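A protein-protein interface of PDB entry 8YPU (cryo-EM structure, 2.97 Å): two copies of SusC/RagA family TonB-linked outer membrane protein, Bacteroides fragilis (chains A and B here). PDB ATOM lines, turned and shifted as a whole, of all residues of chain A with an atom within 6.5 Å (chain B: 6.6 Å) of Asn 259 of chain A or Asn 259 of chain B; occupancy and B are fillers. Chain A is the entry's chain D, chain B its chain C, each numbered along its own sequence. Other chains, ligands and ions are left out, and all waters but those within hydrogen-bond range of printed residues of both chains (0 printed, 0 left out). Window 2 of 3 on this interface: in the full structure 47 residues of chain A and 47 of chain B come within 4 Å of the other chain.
ND2 of Asn 259 of chain B sits at hydrogen-bond distance from OD1 of Asn 259 of chain A.
The side-chain amide nitrogen (ND2) of Asn 259 of chain B is in hydrogen-bond range of the side-chain hydroxyl (OH) of Tyr 264 of chain A (2.5 Å).
OD1 of Asn 259 of chain A is in hydrogen-bond range of OH of Tyr 264 of chain B.
O of Gly 257 of chain B is in hydrogen-bond range of N of Tyr 264 of chain B, 2.9 Å away.
The backbone NH (N) of Tyr 264 of chain A lies within hydrogen-bond range of the backbone carbonyl oxygen (O) of Gly 257 of chain A.
Among the printed residues, merely in contact across the chains: Tyr 264 of chain A with Tyr 264 of chain B, Tyr 264 of chain A with Val 262 of chain B and Val 262 of chain A with Tyr 264 of chain B.
Asn 259 of chain A touches just these residues of chain B: Asn 259 and Tyr 264.
Asn 259 of chain B touches just these residues of chain A: Asn 259 (2.3 Å) and Tyr 264 (2.5 Å).
Printed residues of chain A within 4 Å of Tyr 264 of chain B: Asn 259, Val 262 and Tyr 264.
Printed residues of chain B within 4 Å of Val 262 of chain A: Tyr 264 (3.5 Å).
Printed residues of chain A within 4 Å of Val 262 of chain B: Tyr 264.
Of the printed residues of chain B, Tyr 264 of chain A touches Asn 259 (2.5 Å), Val 262 (3.5 Å) and Tyr 264 (3.4 Å).
The nearest residue of chain A that does not touch Asn 259 of chain B is Gly 258 of chain A (4.4 Å).
The nearest printed residue of chain A that does not touch Val 262 of chain B is Asn 259 of chain A (5.6 Å).
Of the 12 printed residues of chain B, 3 touch a printed residue of chain A.
Of the 12 printed residues of chain A, 3 touch a printed residue of chain B.
Hydrophobic or aromatic side chains of chain A that line the printed part of chain B: Val 262 and Tyr 264.
Asn 259 of chain B touches its own counterpart, Asn 259 of chain A.
Asn 259 of chain A touches Tyr 264 of chain B, and with the chains exchanged Tyr 264 of chain A touches Asn 259 of chain B.
Val 262 of chain A touches Tyr 264 of chain B, and with the chains exchanged Tyr 264 of chain A touches Val 262 of chain B.
Tyr 264 of chain B touches its own counterpart, Tyr 264 of chain A.
12 positions are printed for both chains.
Of the 6 pairs that touch across the chains among the printed residues, 6 have their exchanged pair printed and touching as well.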
ATOM      1  N   LYS A 147      21.607  -6.472   1.234  1.00  0.00           N
ATOM      2  CA  LYS A 147      20.798  -7.406   0.471  1.00  0.00           C
ATOM      3  C   LYS A 147      20.247  -6.717  -0.765  1.00  0.00           C
ATOM      4  O   LYS A 147      20.001  -5.510  -0.762  1.00  0.00           O
ATOM      5  CB  LYS A 147      19.639  -7.937   1.309  1.00  0.00           C
ATOM      6  CG  LYS A 147      20.032  -8.894   2.402  1.00  0.00           C
ATOM      7  CD  LYS A 147      18.812  -9.309   3.192  1.00  0.00           C
ATOM      8  CE  LYS A 147      17.719  -9.832   2.271  1.00  0.00           C
ATOM      9  NZ  LYS A 147      16.546 -10.352   3.026  1.00  0.00           N
ATOM     10  N   VAL A 148      20.036  -7.496  -1.822  1.00  0.00           N
ATOM     11  CA  VAL A 148      19.494  -6.942  -3.056  1.00  0.00           C
ATOM     12  C   VAL A 148      18.058  -6.497  -2.812  1.00  0.00           C
ATOM     13  O   VAL A 148      17.206  -7.288  -2.393  1.00  0.00           O
ATOM     14  CB  VAL A 148      19.581  -7.961  -4.196  1.00  0.00           C
ATOM     15  CG1 VAL A 148      19.002  -7.381  -5.461  1.00  0.00           C
ATOM     16  CG2 VAL A 148      21.018  -8.357  -4.415  1.00  0.00           C
ATOM     17  N   GLY A 149      17.788  -5.233  -3.075  1.00  0.00           N
ATOM     18  CA  GLY A 149      16.490  -4.652  -2.822  1.00  0.00           C
ATOM     19  C   GLY A 149      16.648  -3.187  -2.477  1.00  0.00           C
ATOM     20  O   GLY A 149      17.719  -2.612  -2.624  1.00  0.00           O
ATOM     21  N   GLY A 257      21.848  -2.168   1.230  1.00  0.00           N
ATOM     22  CA  GLY A 257      21.106  -2.304  -0.004  1.00  0.00           C
ATOM     23  C   GLY A 257      21.909  -3.070  -1.027  1.00  0.00           C
ATOM     24  O   GLY A 257      23.030  -3.509  -0.771  1.00  0.00           O
ATOM     25  N   GLY A 258      21.320  -3.206  -2.206  1.00  0.00           N
ATOM     26  CA  GLY A 258      21.984  -3.934  -3.265  1.00  0.00           C
ATOM     27  C   GLY A 258      21.326  -3.725  -4.608  1.00  0.00           C
ATOM     28  O   GLY A 258      20.143  -3.390  -4.702  1.00  0.00           O
ATOM     29  N   ASN A 259      22.121  -3.937  -5.647  1.00  0.00           N
ATOM     30  CA  ASN A 259      21.714  -4.006  -7.039  1.00  0.00           C
ATOM     31  C   ASN A 259      21.817  -5.447  -7.509  1.00  0.00           C
ATOM     32  O   ASN A 259      22.108  -6.361  -6.734  1.00  0.00           O
ATOM     33  CB  ASN A 259      22.594  -3.109  -7.911  1.00  0.00           C
ATOM     34  CG  ASN A 259      22.122  -1.696  -7.951  1.00  0.00           C
ATOM     35  OD1 ASN A 259      22.896  -0.770  -7.732  1.00  0.00           O
ATOM     36  ND2 ASN A 259      20.843  -1.509  -8.240  1.00  0.00           N
ATOM     37  N   GLU A 260      21.601  -5.647  -8.805  1.00  0.00           N
ATOM     38  CA  GLU A 260      21.997  -6.901  -9.422  1.00  0.00           C
ATOM     39  C   GLU A 260      23.505  -6.997  -9.597  1.00  0.00           C
ATOM     40  O   GLU A 260      24.002  -8.069  -9.956  1.00  0.00           O
ATOM     41  CB  GLU A 260      21.299  -7.064 -10.771  1.00  0.00           C
ATOM     42  CG  GLU A 260      21.858  -6.185 -11.872  1.00  0.00           C
ATOM     43  CD  GLU A 260      21.079  -4.901 -12.046  1.00  0.00           C
ATOM     44  OE1 GLU A 260      19.864  -4.901 -11.766  1.00  0.00           O
ATOM     45  OE2 GLU A 260      21.682  -3.890 -12.460  1.00  0.00           O
ATOM     46  N   ARG A 261      24.238  -5.910  -9.352  1.00  0.00           N
ATOM     47  CA  ARG A 261      25.675  -5.888  -9.573  1.00  0.00           C
ATOM     48  C   ARG A 261      26.461  -5.325  -8.394  1.00  0.00           C
ATOM     49  O   ARG A 261      27.640  -5.647  -8.236  1.00  0.00           O
ATOM     50  CB  ARG A 261      25.996  -5.096 -10.839  1.00  0.00           C
ATOM     51  CG  ARG A 261      25.784  -5.885 -12.112  1.00  0.00           C
ATOM     52  CD  ARG A 261      26.232  -5.104 -13.325  1.00  0.00           C
ATOM     53  NE  ARG A 261      27.683  -5.102 -13.449  1.00  0.00           N
ATOM     54  CZ  ARG A 261      28.350  -4.503 -14.424  1.00  0.00           C
ATOM     55  NH1 ARG A 261      27.726  -3.855 -15.391  1.00  0.00           N
ATOM     56  NH2 ARG A 261      29.679  -4.553 -14.428  1.00  0.00           N
ATOM     57  N   VAL A 262      25.848  -4.482  -7.566  1.00  0.00           N
ATOM     58  CA  VAL A 262      26.536  -3.872  -6.430  1.00  0.00           C
ATOM     59  C   VAL A 262      25.694  -4.031  -5.175  1.00  0.00           C
ATOM     60  O   VAL A 262      24.487  -3.773  -5.196  1.00  0.00           O
ATOM     61  CB  VAL A 262      26.842  -2.384  -6.668  1.00  0.00           C
ATOM     62  CG1 VAL A 262      27.662  -1.834  -5.521  1.00  0.00           C
ATOM     63  CG2 VAL A 262      27.566  -2.192  -7.980  1.00  0.00           C
ATOM     64  N   THR A 263      26.333  -4.445  -4.082  1.00  0.00           N
ATOM     65  CA  THR A 263      25.716  -4.457  -2.760  1.00  0.00           C
ATOM     66  C   THR A 263      26.530  -3.590  -1.813  1.00  0.00           C
ATOM     67  O   THR A 263      27.759  -3.656  -1.800  1.00  0.00           O
ATOM     68  CB  THR A 263      25.597  -5.870  -2.189  1.00  0.00           C
ATOM     69  OG1 THR A 263      26.867  -6.525  -2.233  1.00  0.00           O
ATOM     70  CG2 THR A 263      24.592  -6.678  -2.975  1.00  0.00           C
ATOM     71  N   TYR A 264      25.843  -2.781  -1.018  1.00  0.00           N
ATOM     72  CA  TYR A 264      26.489  -1.786  -0.180  1.00  0.00           C
ATOM     73  C   TYR A 264      25.958  -1.857   1.242  1.00  0.00           C
ATOM     74  O   TYR A 264      24.793  -2.191   1.475  1.00  0.00           O
ATOM     75  CB  TYR A 264      26.289  -0.374  -0.742  1.00  0.00           C
ATOM     76  CG  TYR A 264      25.007  -0.207  -1.524  1.00  0.00           C
ATOM     77  CD1 TYR A 264      23.832   0.156  -0.898  1.00  0.00           C
ATOM     78  CD2 TYR A 264      24.979  -0.420  -2.891  1.00  0.00           C
ATOM     79  CE1 TYR A 264      22.672   0.301  -1.612  1.00  0.00           C
ATOM     80  CE2 TYR A 264      23.826  -0.289  -3.605  1.00  0.00           C
ATOM     81  CZ  TYR A 264      22.674   0.077  -2.966  1.00  0.00           C
ATOM     82  OH  TYR A 264      21.511   0.224  -3.685  1.00  0.00           O
ATOM     83  N   LYS A 294      30.113  -6.358  -8.854  1.00  0.00           N
ATOM     84  CA  LYS A 294      30.262  -7.420  -9.843  1.00  0.00           C
ATOM     85  C   LYS A 294      30.813  -6.765 -11.100  1.00  0.00           C
ATOM     86  O   LYS A 294      30.072  -6.279 -11.952  1.00  0.00           O
ATOM     87  CB  LYS A 294      28.936  -8.121 -10.091  1.00  0.00           C
ATOM     88  CG  LYS A 294      28.736  -9.352  -9.242  1.00  0.00           C
ATOM     89  CD  LYS A 294      27.432 -10.040  -9.568  1.00  0.00           C
ATOM     90  CE  LYS A 294      26.434  -9.882  -8.441  1.00  0.00           C
ATOM     91  NZ  LYS A 294      25.190 -10.654  -8.688  1.00  0.00           N
ATOM     92  N   LYS B 147      27.770   7.879 -10.612  1.00  0.00           N
ATOM     93  CA  LYS B 147      26.681   8.281 -11.484  1.00  0.00           C
ATOM     94  C   LYS B 147      25.668   7.154 -11.592  1.00  0.00           C
ATOM     95  O   LYS B 147      26.018   5.976 -11.505  1.00  0.00           O
ATOM     96  CB  LYS B 147      27.195   8.631 -12.877  1.00  0.00           C
ATOM     97  CG  LYS B 147      27.973   9.917 -12.962  1.00  0.00           C
ATOM     98  CD  LYS B 147      28.468  10.130 -14.373  1.00  0.00           C
ATOM     99  CE  LYS B 147      27.325  10.026 -15.373  1.00  0.00           C
ATOM    100  NZ  LYS B 147      27.759  10.340 -16.763  1.00  0.00           N
ATOM    101  N   VAL B 148      24.408   7.521 -11.803  1.00  0.00           N
ATOM    102  CA  VAL B 148      23.356   6.522 -11.937  1.00  0.00           C
ATOM    103  C   VAL B 148      23.580   5.735 -13.221  1.00  0.00           C
ATOM    104  O   VAL B 148      23.644   6.305 -14.317  1.00  0.00           O
ATOM    105  CB  VAL B 148      21.972   7.178 -11.912  1.00  0.00           C
ATOM    106  CG1 VAL B 148      20.895   6.133 -12.050  1.00  0.00           C
ATOM    107  CG2 VAL B 148      21.796   7.943 -10.626  1.00  0.00           C
ATOM    108  N   GLY B 149      23.693   4.427 -13.092  1.00  0.00           N
ATOM    109  CA  GLY B 149      23.981   3.564 -14.213  1.00  0.00           C
ATOM    110  C   GLY B 149      24.772   2.364 -13.739  1.00  0.00           C
ATOM    111  O   GLY B 149      24.915   2.129 -12.546  1.00  0.00           O
ATOM    112  N   GLY B 257      29.137   4.020  -9.236  1.00  0.00           N
ATOM    113  CA  GLY B 257      27.853   3.579  -9.735  1.00  0.00           C
ATOM    114  C   GLY B 257      26.731   4.276  -9.005  1.00  0.00           C
ATOM    115  O   GLY B 257      26.952   5.086  -8.104  1.00  0.00           O
ATOM    116  N   GLY B 258      25.516   3.926  -9.397  1.00  0.00           N
ATOM    117  CA  GLY B 258      24.357   4.553  -8.801  1.00  0.00           C
ATOM    118  C   GLY B 258      23.089   3.779  -9.063  1.00  0.00           C
ATOM    119  O   GLY B 258      22.999   2.985 -10.002  1.00  0.00           O
ATOM    120  N   ASN B 259      22.107   4.035  -8.214  1.00  0.00           N
ATOM    121  CA  ASN B 259      20.741   3.550  -8.318  1.00  0.00           C
ATOM    122  C   ASN B 259      19.815   4.737  -8.534  1.00  0.00           C
ATOM    123  O   ASN B 259      20.251   5.880  -8.673  1.00  0.00           O
ATOM    124  CB  ASN B 259      20.329   2.804  -7.050  1.00  0.00           C
ATOM    125  CG  ASN B 259      20.499   1.329  -7.165  1.00  0.00           C
ATOM    126  OD1 ASN B 259      20.171   0.738  -8.188  1.00  0.00           O
ATOM    127  ND2 ASN B 259      21.024   0.713  -6.117  1.00  0.00           N
ATOM    128  N   GLU B 260      18.516   4.459  -8.531  1.00  0.00           N
ATOM    129  CA  GLU B 260      17.561   5.543  -8.373  1.00  0.00           C
ATOM    130  C   GLU B 260      17.510   6.045  -6.939  1.00  0.00           C
ATOM    131  O   GLU B 260      16.874   7.072  -6.682  1.00  0.00           O
ATOM    132  CB  GLU B 260      16.168   5.099  -8.823  1.00  0.00           C
ATOM    133  CG  GLU B 260      15.472   4.144  -7.872  1.00  0.00           C
ATOM    134  CD  GLU B 260      15.681   2.693  -8.247  1.00  0.00           C
ATOM    135  OE1 GLU B 260      15.810   2.405  -9.454  1.00  0.00           O
ATOM    136  OE2 GLU B 260      15.710   1.840  -7.337  1.00  0.00           O
ATOM    137  N   ARG B 261      18.164   5.351  -6.008  1.00  0.00           N
ATOM    138  CA  ARG B 261      18.147   5.720  -4.601  1.00  0.00           C
ATOM    139  C   ARG B 261      19.507   5.721  -3.920  1.00  0.00           C
ATOM    140  O   ARG B 261      19.638   6.369  -2.879  1.00  0.00           O
ATOM    141  CB  ARG B 261      17.207   4.795  -3.818  1.00  0.00           C
ATOM    142  CG  ARG B 261      15.743   5.127  -3.996  1.00  0.00           C
ATOM    143  CD  ARG B 261      14.872   4.229  -3.150  1.00  0.00           C
ATOM    144  NE  ARG B 261      14.897   4.631  -1.750  1.00  0.00           N
ATOM    145  CZ  ARG B 261      14.238   4.011  -0.782  1.00  0.00           C
ATOM    146  NH1 ARG B 261      13.476   2.960  -1.029  1.00  0.00           N
ATOM    147  NH2 ARG B 261      14.349   4.455   0.465  1.00  0.00           N
ATOM    148  N   VAL B 262      20.512   5.021  -4.441  1.00  0.00           N
ATOM    149  CA  VAL B 262      21.839   4.989  -3.831  1.00  0.00           C
ATOM    150  C   VAL B 262      22.894   5.211  -4.903  1.00  0.00           C
ATOM    151  O   VAL B 262      22.842   4.591  -5.968  1.00  0.00           O
ATOM    152  CB  VAL B 262      22.110   3.665  -3.098  1.00  0.00           C
ATOM    153  CG1 VAL B 262      23.450   3.726  -2.395  1.00  0.00           C
ATOM    154  CG2 VAL B 262      21.006   3.363  -2.113  1.00  0.00           C
ATOM    155  N   THR B 263      23.855   6.087  -4.616  1.00  0.00           N
ATOM    156  CA  THR B 263      25.040   6.256  -5.448  1.00  0.00           C
ATOM    157  C   THR B 263      26.283   5.964  -4.622  1.00  0.00           C
ATOM    158  O   THR B 263      26.399   6.411  -3.481  1.00  0.00           O
ATOM    159  CB  THR B 263      25.134   7.660  -6.046  1.00  0.00           C
ATOM    160  OG1 THR B 263      25.151   8.637  -5.002  1.00  0.00           O
ATOM    161  CG2 THR B 263      23.967   7.926  -6.964  1.00  0.00           C
ATOM    162  N   TYR B 264      27.213   5.218  -5.203  1.00  0.00           N
ATOM    163  CA  TYR B 264      28.376   4.727  -4.484  1.00  0.00           C
ATOM    164  C   TYR B 264      29.644   5.004  -5.270  1.00  0.00           C
ATOM    165  O   TYR B 264      29.646   5.013  -6.503  1.00  0.00           O
ATOM    166  CB  TYR B 264      28.255   3.226  -4.196  1.00  0.00           C
ATOM    167  CG  TYR B 264      27.435   2.472  -5.217  1.00  0.00           C
ATOM    168  CD1 TYR B 264      28.018   1.938  -6.347  1.00  0.00           C
ATOM    169  CD2 TYR B 264      26.072   2.303  -5.044  1.00  0.00           C
ATOM    170  CE1 TYR B 264      27.268   1.260  -7.272  1.00  0.00           C
ATOM    171  CE2 TYR B 264      25.317   1.639  -5.965  1.00  0.00           C
ATOM    172  CZ  TYR B 264      25.918   1.114  -7.075  1.00  0.00           C
ATOM    173  OH  TYR B 264      25.163   0.432  -8.001  1.00  0.00           O
ATOM    174  N   LYS B 294      19.111   7.722  -0.662  1.00  0.00           N
ATOM    175  CA  LYS B 294      17.862   8.477  -0.627  1.00  0.00           C
ATOM    176  C   LYS B 294      16.921   7.715   0.294  1.00  0.00           C
ATOM    177  O   LYS B 294      16.204   6.808  -0.126  1.00  0.00           O
ATOM    178  CB  LYS B 294      17.289   8.643  -2.025  1.00  0.00           C
ATOM    179  CG  LYS B 294      17.690   9.933  -2.695  1.00  0.00           C
ATOM    180  CD  LYS B 294      17.038  10.072  -4.051  1.00  0.00           C
ATOM    181  CE  LYS B 294      18.053   9.924  -5.163  1.00  0.00           C
ATOM    182  NZ  LYS B 294      17.456  10.185  -6.498  1.00  0.00           N
